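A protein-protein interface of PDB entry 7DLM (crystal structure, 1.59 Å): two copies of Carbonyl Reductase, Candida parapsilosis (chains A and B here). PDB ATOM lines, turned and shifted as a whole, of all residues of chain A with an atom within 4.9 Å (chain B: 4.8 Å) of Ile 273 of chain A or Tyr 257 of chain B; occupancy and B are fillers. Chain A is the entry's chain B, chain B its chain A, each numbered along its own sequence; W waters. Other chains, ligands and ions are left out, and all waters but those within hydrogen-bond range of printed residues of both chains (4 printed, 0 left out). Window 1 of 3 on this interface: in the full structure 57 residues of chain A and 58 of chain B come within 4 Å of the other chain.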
ATOM      1  N   ILE A 215      10.810  -7.891 -25.447  1.00  0.00           N
ATOM      2  CA  ILE A 215      12.222  -7.514 -25.413  1.00  0.00           C
ATOM      3  C   ILE A 215      13.017  -8.776 -25.120  1.00  0.00           C
ATOM      4  O   ILE A 215      12.707  -9.496 -24.163  1.00  0.00           O
ATOM      5  CB  ILE A 215      12.507  -6.447 -24.335  1.00  0.00           C
ATOM      6  CG1 ILE A 215      11.779  -5.124 -24.627  1.00  0.00           C
ATOM      7  CG2 ILE A 215      14.029  -6.267 -24.180  1.00  0.00           C
ATOM      8  CD1 ILE A 215      12.493  -4.185 -25.581  1.00  0.00           C
ATOM      9  N   SER A 216      14.029  -9.071 -25.945  1.00  0.00           N
ATOM     10  CA  SER A 216      14.901 -10.213 -25.660  1.00  0.00           C
ATOM     11  C   SER A 216      16.306  -9.712 -25.339  1.00  0.00           C
ATOM     12  O   SER A 216      17.102  -9.462 -26.262  1.00  0.00           O
ATOM     13  CB  SER A 216      14.934 -11.180 -26.848  1.00  0.00           C
ATOM     14  OG  SER A 216      13.718 -11.905 -26.911  1.00  0.00           O
ATOM     15  N   PRO A 217      16.660  -9.526 -24.070  1.00  0.00           N
ATOM     16  CA  PRO A 217      18.036  -9.117 -23.753  1.00  0.00           C
ATOM     17  C   PRO A 217      19.017 -10.261 -23.938  1.00  0.00           C
ATOM     18  O   PRO A 217      18.675 -11.437 -23.778  1.00  0.00           O
ATOM     19  CB  PRO A 217      17.966  -8.702 -22.274  1.00  0.00           C
ATOM     20  CG  PRO A 217      16.464  -8.711 -21.909  1.00  0.00           C
ATOM     21  CD  PRO A 217      15.839  -9.690 -22.855  1.00  0.00           C
ATOM     22  N   GLY A 218      20.254  -9.890 -24.283  1.00  0.00           N
ATOM     23  CA  GLY A 218      21.402 -10.767 -24.120  1.00  0.00           C
ATOM     24  C   GLY A 218      21.936 -10.694 -22.702  1.00  0.00           C
ATOM     25  O   GLY A 218      21.184 -10.465 -21.749  1.00  0.00           O
ATOM     26  N   ILE A 220      23.242  -9.209 -19.579  1.00  0.00           N
ATOM     27  CA  ILE A 220      23.150  -7.888 -18.969  1.00  0.00           C
ATOM     28  C   ILE A 220      23.732  -7.987 -17.565  1.00  0.00           C
ATOM     29  O   ILE A 220      23.483  -8.963 -16.848  1.00  0.00           O
ATOM     30  CB  ILE A 220      21.690  -7.378 -18.925  1.00  0.00           C
ATOM     31  CG1 ILE A 220      21.007  -7.503 -20.300  1.00  0.00           C
ATOM     32  CG2 ILE A 220      21.608  -5.941 -18.380  1.00  0.00           C
ATOM     33  CD1 ILE A 220      21.603  -6.621 -21.379  1.00  0.00           C
ATOM     34  N   GLU A 250      21.099   0.279 -21.156  1.00  0.00           N
ATOM     35  CA  GLU A 250      21.079   0.016 -22.586  1.00  0.00           C
ATOM     36  C   GLU A 250      19.829  -0.748 -23.008  1.00  0.00           C
ATOM     37  O   GLU A 250      19.665  -1.035 -24.204  1.00  0.00           O
ATOM     38  CB  GLU A 250      22.335  -0.761 -22.988  1.00  0.00           C
ATOM     39  CG  GLU A 250      23.627   0.029 -22.730  1.00  0.00           C
ATOM     40  CD  GLU A 250      24.859  -0.697 -23.233  1.00  0.00           C
ATOM     41  OE1 GLU A 250      25.228  -1.737 -22.627  1.00  0.00           O
ATOM     42  OE2 GLU A 250      25.445  -0.250 -24.250  1.00  0.00           O
ATOM     43  N   LEU A 251      18.949  -1.077 -22.056  1.00  0.00           N
ATOM     44  CA  LEU A 251      17.669  -1.721 -22.342  1.00  0.00           C
ATOM     45  C   LEU A 251      16.497  -0.762 -22.293  1.00  0.00           C
ATOM     46  O   LEU A 251      15.491  -0.991 -22.979  1.00  0.00           O
ATOM     47  CB  LEU A 251      17.381  -2.850 -21.341  1.00  0.00           C
ATOM     48  CG  LEU A 251      18.338  -4.028 -21.220  1.00  0.00           C
ATOM     49  CD1 LEU A 251      17.932  -4.896 -20.044  1.00  0.00           C
ATOM     50  CD2 LEU A 251      18.376  -4.823 -22.517  1.00  0.00           C
ATOM     51  N   GLY A 253      15.758   2.178 -23.385  1.00  0.00           N
ATOM     52  CA  GLY A 253      15.286   2.788 -24.617  1.00  0.00           C
ATOM     53  C   GLY A 253      14.325   1.891 -25.380  1.00  0.00           C
ATOM     54  O   GLY A 253      13.346   2.366 -25.955  1.00  0.00           O
ATOM     55  N   GLY A 254      14.610   0.587 -25.412  1.00  0.00           N
ATOM     56  CA  GLY A 254      13.739  -0.338 -26.130  1.00  0.00           C
ATOM     57  C   GLY A 254      12.422  -0.576 -25.412  1.00  0.00           C
ATOM     58  O   GLY A 254      11.365  -0.679 -26.047  1.00  0.00           O
ATOM     59  N   TYR A 257      10.421   2.554 -26.171  1.00  0.00           N
ATOM     60  CA  TYR A 257       9.939   2.479 -27.546  1.00  0.00           C
ATOM     61  C   TYR A 257       8.636   1.683 -27.626  1.00  0.00           C
ATOM     62  O   TYR A 257       7.626   2.170 -28.157  1.00  0.00           O
ATOM     63  CB  TYR A 257      11.036   1.853 -28.430  1.00  0.00           C
ATOM     64  CG  TYR A 257      10.531   1.538 -29.814  1.00  0.00           C
ATOM     65  CD1 TYR A 257      10.152   2.567 -30.675  1.00  0.00           C
ATOM     66  CD2 TYR A 257      10.372   0.212 -30.237  1.00  0.00           C
ATOM     67  CE1 TYR A 257       9.652   2.294 -31.937  1.00  0.00           C
ATOM     68  CE2 TYR A 257       9.877  -0.081 -31.508  1.00  0.00           C
ATOM     69  CZ  TYR A 257       9.507   0.976 -32.342  1.00  0.00           C
ATOM     70  OH  TYR A 257       8.988   0.708 -33.582  1.00  0.00           O
ATOM     71  N   VAL A 271      12.151  -7.496 -30.057  1.00  0.00           N
ATOM     72  CA  VAL A 271      13.223  -6.498 -30.092  1.00  0.00           C
ATOM     73  C   VAL A 271      14.418  -7.085 -29.338  1.00  0.00           C
ATOM     74  O   VAL A 271      14.405  -7.172 -28.107  1.00  0.00           O
ATOM     75  CB  VAL A 271      12.767  -5.165 -29.494  1.00  0.00           C
ATOM     76  CG1 VAL A 271      13.923  -4.186 -29.424  1.00  0.00           C
ATOM     77  CG2 VAL A 271      11.615  -4.574 -30.317  1.00  0.00           C
ATOM     78  N   VAL A 272      15.440  -7.539 -30.086  1.00  0.00           N
ATOM     79  CA  VAL A 272      16.618  -8.190 -29.499  1.00  0.00           C
ATOM     80  C   VAL A 272      17.678  -7.149 -29.154  1.00  0.00           C
ATOM     81  O   VAL A 272      18.035  -6.312 -29.992  1.00  0.00           O
ATOM     82  CB  VAL A 272      17.182  -9.251 -30.458  1.00  0.00           C
ATOM     83  CG1 VAL A 272      18.394  -9.945 -29.844  1.00  0.00           C
ATOM     84  CG2 VAL A 272      16.104 -10.253 -30.762  1.00  0.00           C
ATOM     85  N   ILE A 273      18.166  -7.189 -27.907  1.00  0.00           N
ATOM     86  CA  ILE A 273      19.145  -6.222 -27.391  1.00  0.00           C
ATOM     87  C   ILE A 273      20.268  -7.040 -26.758  1.00  0.00           C
ATOM     88  O   ILE A 273      20.271  -7.286 -25.545  1.00  0.00           O
ATOM     89  CB  ILE A 273      18.533  -5.241 -26.384  1.00  0.00           C
ATOM     90  CG1 ILE A 273      17.308  -4.553 -26.994  1.00  0.00           C
ATOM     91  CG2 ILE A 273      19.565  -4.195 -25.976  1.00  0.00           C
ATOM     92  CD1 ILE A 273      16.559  -3.573 -26.032  1.00  0.00           C
ATOM     93  N   ASP A 274      21.250  -7.464 -27.581  1.00  0.00           N
ATOM     94  CA  ASP A 274      22.160  -8.524 -27.158  1.00  0.00           C
ATOM     95  C   ASP A 274      23.606  -8.322 -27.598  1.00  0.00           C
ATOM     96  O   ASP A 274      24.384  -9.278 -27.557  1.00  0.00           O
ATOM     97  CB  ASP A 274      21.682  -9.901 -27.661  1.00  0.00           C
ATOM     98  CG  ASP A 274      21.773 -10.061 -29.184  1.00  0.00           C
ATOM     99  OD1 ASP A 274      22.048  -9.076 -29.909  1.00  0.00           O
ATOM    100  OD2 ASP A 274      21.558 -11.205 -29.644  1.00  0.00           O
ATOM    101  N   GLY A 275      23.992  -7.116 -28.009  1.00  0.00           N
ATOM    102  CA  GLY A 275      25.360  -6.912 -28.463  1.00  0.00           C
ATOM    103  C   GLY A 275      25.735  -7.739 -29.668  1.00  0.00           C
ATOM    104  O   GLY A 275      26.927  -7.944 -29.924  1.00  0.00           O
ATOM    105  N   PHE B  31      17.779   9.599 -26.618  1.00  0.00           N
ATOM    106  CA  PHE B  31      17.259   9.701 -27.975  1.00  0.00           C
ATOM    107  C   PHE B  31      17.698  10.977 -28.688  1.00  0.00           C
ATOM    108  O   PHE B  31      17.354  11.171 -29.856  1.00  0.00           O
ATOM    109  CB  PHE B  31      15.722   9.622 -27.966  1.00  0.00           C
ATOM    110  CG  PHE B  31      15.191   8.257 -27.601  1.00  0.00           C
ATOM    111  CD1 PHE B  31      15.041   7.889 -26.265  1.00  0.00           C
ATOM    112  CD2 PHE B  31      14.873   7.327 -28.590  1.00  0.00           C
ATOM    113  CE1 PHE B  31      14.566   6.627 -25.929  1.00  0.00           C
ATOM    114  CE2 PHE B  31      14.392   6.077 -28.263  1.00  0.00           C
ATOM    115  CZ  PHE B  31      14.237   5.723 -26.940  1.00  0.00           C
ATOM    116  N   GLY B 253       9.885   6.480 -34.872  1.00  0.00           N
ATOM    117  CA  GLY B 253      10.360   6.075 -33.553  1.00  0.00           C
ATOM    118  C   GLY B 253      11.440   5.007 -33.611  1.00  0.00           C
ATOM    119  O   GLY B 253      12.428   5.070 -32.879  1.00  0.00           O
ATOM    120  N   GLY B 254      11.264   4.006 -34.478  1.00  0.00           N
ATOM    121  CA  GLY B 254      12.257   2.936 -34.572  1.00  0.00           C
ATOM    122  C   GLY B 254      13.566   3.400 -35.187  1.00  0.00           C
ATOM    123  O   GLY B 254      14.643   2.984 -34.754  1.00  0.00           O
ATOM    124  N   TYR B 255      13.488   4.255 -36.215  1.00  0.00           N
ATOM    125  CA  TYR B 255      14.699   4.815 -36.815  1.00  0.00           C
ATOM    126  C   TYR B 255      15.463   5.677 -35.816  1.00  0.00           C
ATOM    127  O   TYR B 255      16.698   5.696 -35.826  1.00  0.00           O
ATOM    128  CB  TYR B 255      14.355   5.622 -38.078  1.00  0.00           C
ATOM    129  CG  TYR B 255      14.110   4.770 -39.313  1.00  0.00           C
ATOM    130  CD1 TYR B 255      15.159   4.418 -40.167  1.00  0.00           C
ATOM    131  CD2 TYR B 255      12.830   4.318 -39.626  1.00  0.00           C
ATOM    132  CE1 TYR B 255      14.929   3.636 -41.304  1.00  0.00           C
ATOM    133  CE2 TYR B 255      12.591   3.543 -40.762  1.00  0.00           C
ATOM    134  CZ  TYR B 255      13.646   3.190 -41.581  1.00  0.00           C
ATOM    135  OH  TYR B 255      13.388   2.434 -42.706  1.00  0.00           O
ATOM    136  N   LEU B 256      14.751   6.404 -34.944  1.00  0.00           N
ATOM    137  CA  LEU B 256      15.451   7.221 -33.952  1.00  0.00           C
ATOM    138  C   LEU B 256      16.021   6.352 -32.839  1.00  0.00           C
ATOM    139  O   LEU B 256      17.122   6.621 -32.337  1.00  0.00           O
ATOM    140  CB  LEU B 256      14.519   8.294 -33.374  1.00  0.00           C
ATOM    141  CG  LEU B 256      15.199   9.221 -32.349  1.00  0.00           C
ATOM    142  CD1 LEU B 256      16.324  10.023 -33.003  1.00  0.00           C
ATOM    143  CD2 LEU B 256      14.154  10.157 -31.714  1.00  0.00           C
ATOM    144  N   TYR B 257      15.282   5.312 -32.436  1.00  0.00           N
ATOM    145  CA  TYR B 257      15.809   4.334 -31.489  1.00  0.00           C
ATOM    146  C   TYR B 257      17.174   3.826 -31.932  1.00  0.00           C
ATOM    147  O   TYR B 257      18.138   3.858 -31.159  1.00  0.00           O
ATOM    148  CB  TYR B 257      14.816   3.164 -31.329  1.00  0.00           C
ATOM    149  CG  TYR B 257      15.405   2.017 -30.530  1.00  0.00           C
ATOM    150  CD1 TYR B 257      15.643   2.138 -29.153  1.00  0.00           C
ATOM    151  CD2 TYR B 257      15.760   0.828 -31.153  1.00  0.00           C
ATOM    152  CE1 TYR B 257      16.225   1.096 -28.433  1.00  0.00           C
ATOM    153  CE2 TYR B 257      16.344  -0.210 -30.441  1.00  0.00           C
ATOM    154  CZ  TYR B 257      16.572  -0.073 -29.081  1.00  0.00           C
ATOM    155  OH  TYR B 257      17.163  -1.120 -28.388  1.00  0.00           O
ATOM    156  N   LEU B 258      17.272   3.338 -33.177  1.00  0.00           N
ATOM    157  CA  LEU B 258      18.518   2.735 -33.659  1.00  0.00           C
ATOM    158  C   LEU B 258      19.613   3.768 -33.908  1.00  0.00           C
ATOM    159  O   LEU B 258      20.802   3.450 -33.768  1.00  0.00           O
ATOM    160  CB  LEU B 258      18.249   1.947 -34.940  1.00  0.00           C
ATOM    161  CG  LEU B 258      17.413   0.670 -34.807  1.00  0.00           C
ATOM    162  CD1 LEU B 258      17.175   0.075 -36.206  1.00  0.00           C
ATOM    163  CD2 LEU B 258      18.059  -0.338 -33.869  1.00  0.00           C
ATOM    164  N   ALA B 259      19.244   4.999 -34.269  1.00  0.00           N
ATOM    165  CA  ALA B 259      20.241   6.008 -34.613  1.00  0.00           C
ATOM    166  C   ALA B 259      20.952   6.562 -33.393  1.00  0.00           C
ATOM    167  O   ALA B 259      22.106   7.005 -33.504  1.00  0.00           O
ATOM    168  CB  ALA B 259      19.595   7.182 -35.354  1.00  0.00           C
ATOM    169  N   SER B 260      20.281   6.570 -32.249  1.00  0.00           N
ATOM    170  CA  SER B 260      20.693   7.328 -31.076  1.00  0.00           C
ATOM    171  C   SER B 260      21.364   6.433 -30.025  1.00  0.00           C
ATOM    172  O   SER B 260      21.513   5.218 -30.191  1.00  0.00           O
ATOM    173  CB  SER B 260      19.487   8.043 -30.457  1.00  0.00           C
ATOM    174  OG  SER B 260      18.547   7.102 -29.920  1.00  0.00           O
ATOM    175  N   ALA B 262      20.011   5.510 -27.444  1.00  0.00           N
ATOM    176  CA  ALA B 262      19.034   4.622 -26.833  1.00  0.00           C
ATOM    177  C   ALA B 262      19.318   3.158 -27.107  1.00  0.00           C
ATOM    178  O   ALA B 262      18.699   2.307 -26.465  1.00  0.00           O
ATOM    179  CB  ALA B 262      17.637   4.963 -27.339  1.00  0.00           C
ATOM    180  N   SER B 263      20.226   2.841 -28.033  1.00  0.00           N
ATOM    181  CA  SER B 263      20.406   1.478 -28.525  1.00  0.00           C
ATOM    182  C   SER B 263      21.878   1.078 -28.583  1.00  0.00           C
ATOM    183  O   SER B 263      22.300   0.356 -29.499  1.00  0.00           O
ATOM    184  CB  SER B 263      19.784   1.331 -29.914  1.00  0.00           C
ATOM    185  OG  SER B 263      20.344   2.268 -30.839  1.00  0.00           O
ATOM    186  N   PHE B 265      23.674  -1.085 -27.064  1.00  0.00           N
ATOM    187  CA  PHE B 265      23.934  -2.522 -27.031  1.00  0.00           C
ATOM    188  C   PHE B 265      23.175  -3.258 -28.127  1.00  0.00           C
ATOM    189  O   PHE B 265      23.157  -4.488 -28.141  1.00  0.00           O
ATOM    190  CB  PHE B 265      23.580  -3.101 -25.646  1.00  0.00           C
ATOM    191  CG  PHE B 265      24.245  -4.442 -25.313  1.00  0.00           C
ATOM    192  CD1 PHE B 265      23.464  -5.525 -24.920  1.00  0.00           C
ATOM    193  CD2 PHE B 265      25.627  -4.621 -25.382  1.00  0.00           C
ATOM    194  CE1 PHE B 265      24.034  -6.744 -24.593  1.00  0.00           C
ATOM    195  CE2 PHE B 265      26.209  -5.849 -25.045  1.00  0.00           C
ATOM    196  CZ  PHE B 265      25.415  -6.912 -24.656  1.00  0.00           C
ATOM    197  N   THR B 266      22.543  -2.533 -29.051  1.00  0.00           N
ATOM    198  CA  THR B 266      21.734  -3.141 -30.100  1.00  0.00           C
ATOM    199  C   THR B 266      22.526  -3.128 -31.397  1.00  0.00           C
ATOM    200  O   THR B 266      22.779  -2.060 -31.961  1.00  0.00           O
ATOM    201  CB  THR B 266      20.426  -2.368 -30.246  1.00  0.00           C
ATOM    202  OG1 THR B 266      19.792  -2.300 -28.962  1.00  0.00           O
ATOM    203  CG2 THR B 266      19.499  -3.056 -31.218  1.00  0.00           C
HETATM  204  O   HOH W   1       8.373   3.047 -34.813  1.00  0.00           O
HETATM  205  O   HOH W   2      20.931  -1.023 -26.632  1.00  0.00           O
HETATM  206  O   HOH W   3      18.567   2.137 -23.566  1.00  0.00           O
HETATM  207  O   HOH W   4      17.599  -0.161 -25.866  1.00  0.00           O
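The backbone NH (N) of Phe 265 of chain B lies within hydrogen-bond range of the side-chain carboxylate (OE2) of Glu 250 of chain A.
The backbone carbonyl oxygen (O) of Phe 265 of chain B is in hydrogen-bond range of the backbone NH (N) of Gly 275 of chain A, 2.8 Å away.
The backbone carbonyl oxygen (O) of Tyr 257 of chain B lies within hydrogen-bond range of the side-chain hydroxyl (OG) of Ser 260 of chain B (3.5 Å).
O of Tyr 257 of chain B sits at hydrogen-bond distance from OG of Ser 263 of chain B.
The side-chain hydroxyl of Tyr 257 of chain B is in hydrogen-bond range of the side-chain hydroxyl of Thr 266 of chain B, at 2.9 Å.
The backbone NH (N) of Ala 262 of chain B lies close to the side-chain hydroxyl (OG) of Ser 260 of chain B (3.3 Å).
The backbone carbonyl oxygen (O) of Ser 216 of chain A sits at hydrogen-bond distance from the backbone NH (N) of Ile 273 of chain A, 3.0 Å away.
O of Ile 273 of chain A lies within hydrogen-bond range of N of Gly 218 of chain A (2.9 Å).
Gly 253 of chain A touches Phe 31 of chain B (O to CZ, 3.6 Å).
C of Gly 253 of chain A touches CE1 of Tyr 257 of chain B, at 3.7 Å.
Ala 262 of chain B touches Gly 253 of chain A (O to CA, 3.9 Å).
Gly 254 of chain A touches Tyr 257 of chain B (N to CE1, 3.5 Å).
Tyr 257 of chain A touches Gly 253 of chain B (CE1 to C, 3.7 Å).
CE1 of Tyr 257 of chain A touches N of Gly 254 of chain B, at 3.5 Å.
Thr 266 of chain B touches Val 272 of chain A.
CD1 of Ile 273 of chain A touches OH of Tyr 257 of chain B, 3.5 Å away.
Thr 266 of chain B touches Ile 273 of chain A.
Asp 274 of chain A touches Phe 265 of chain B (C to CE1, 3.4 Å).
Of the printed residues of chain B, Gly 254 of chain A touches Tyr 257 (3.5 Å).
Printed residues of chain B within 4 Å of Tyr 257 of chain A: Gly 253 and Gly 254.
Ile 273 of chain A touches just these residues of chain B: Tyr 257, Phe 265 and Thr 266.
Printed residues of chain A within 4 Å of Gly 253 of chain B: Tyr 257 (3.7 Å).
Printed residues of chain A within 4 Å of Gly 254 of chain B: Tyr 257 (3.5 Å).
Of the printed residues of chain A, Tyr 257 of chain B touches Gly 253, Gly 254 and Ile 273.
Leu 258 of chain B touches none of the printed residues of chain A.
The nearest residue of chain A that does not touch Tyr 257 of chain B is Val 271 of chain A (4.6 Å).
Hydrophobic or aromatic side chains of chain B within 4 Å of the printed part of chain A: Phe 31, Tyr 257 and Phe 265.
Hydrophobic or aromatic side chains of chain A within 4 Å of the printed part of chain B: Tyr 257 and Ile 273.
Along chain A the printed residues that touch a printed residue of chain B span positions 250 to 275.
Among the printed residues, no Asp or Glu carboxylate lies within 4 Å of a Lys or Arg side-chain nitrogen of the other chain.
Gly 253 of chain A touches Tyr 257 of chain B, and with the chains exchanged Tyr 257 of chain A touches Gly 253 of chain B.
Gly 254 of chain A touches Tyr 257 of chain B, and with the chains exchanged Tyr 257 of chain A touches Gly 254 of chain B.
Positions printed for both chains: 253, 254 and 257.
Of the 13 pairs that touch across the chains among the printed residues, 4 have their exchanged pair printed and touching as well.
Water W1 bridges the side-chain hydroxyl of Tyr 257 of chain A and the backbone NH of Gly 254 of chain B.
Water W4 lies within hydrogen-bond range of the side-chain hydroxyl (OH) of Tyr 257 of chain B (2.7 Å), the backbone carbonyl oxygen (O) of Ala 262 of chain B (2.8 Å), the backbone carbonyl oxygen (O) of Glu 250 of chain A (2.8 Å) and the backbone NH (N) of Gly 254 of chain A (3.1 Å).
Water W2 lies within hydrogen-bond range of the backbone carbonyl oxygen of Glu 250 of chain A, the backbone NH of Phe 265 of chain B, the side-chain hydroxyl of Thr 266 of chain B and the backbone carbonyl oxygen of Ser 263 of chain B.
Water W3 lies within hydrogen-bond range of N of Gly 253 of chain A (2.8 Å), O of Ala 262 of chain B (2.9 Å) and O of Glu 250 of chain A (3.4 Å).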
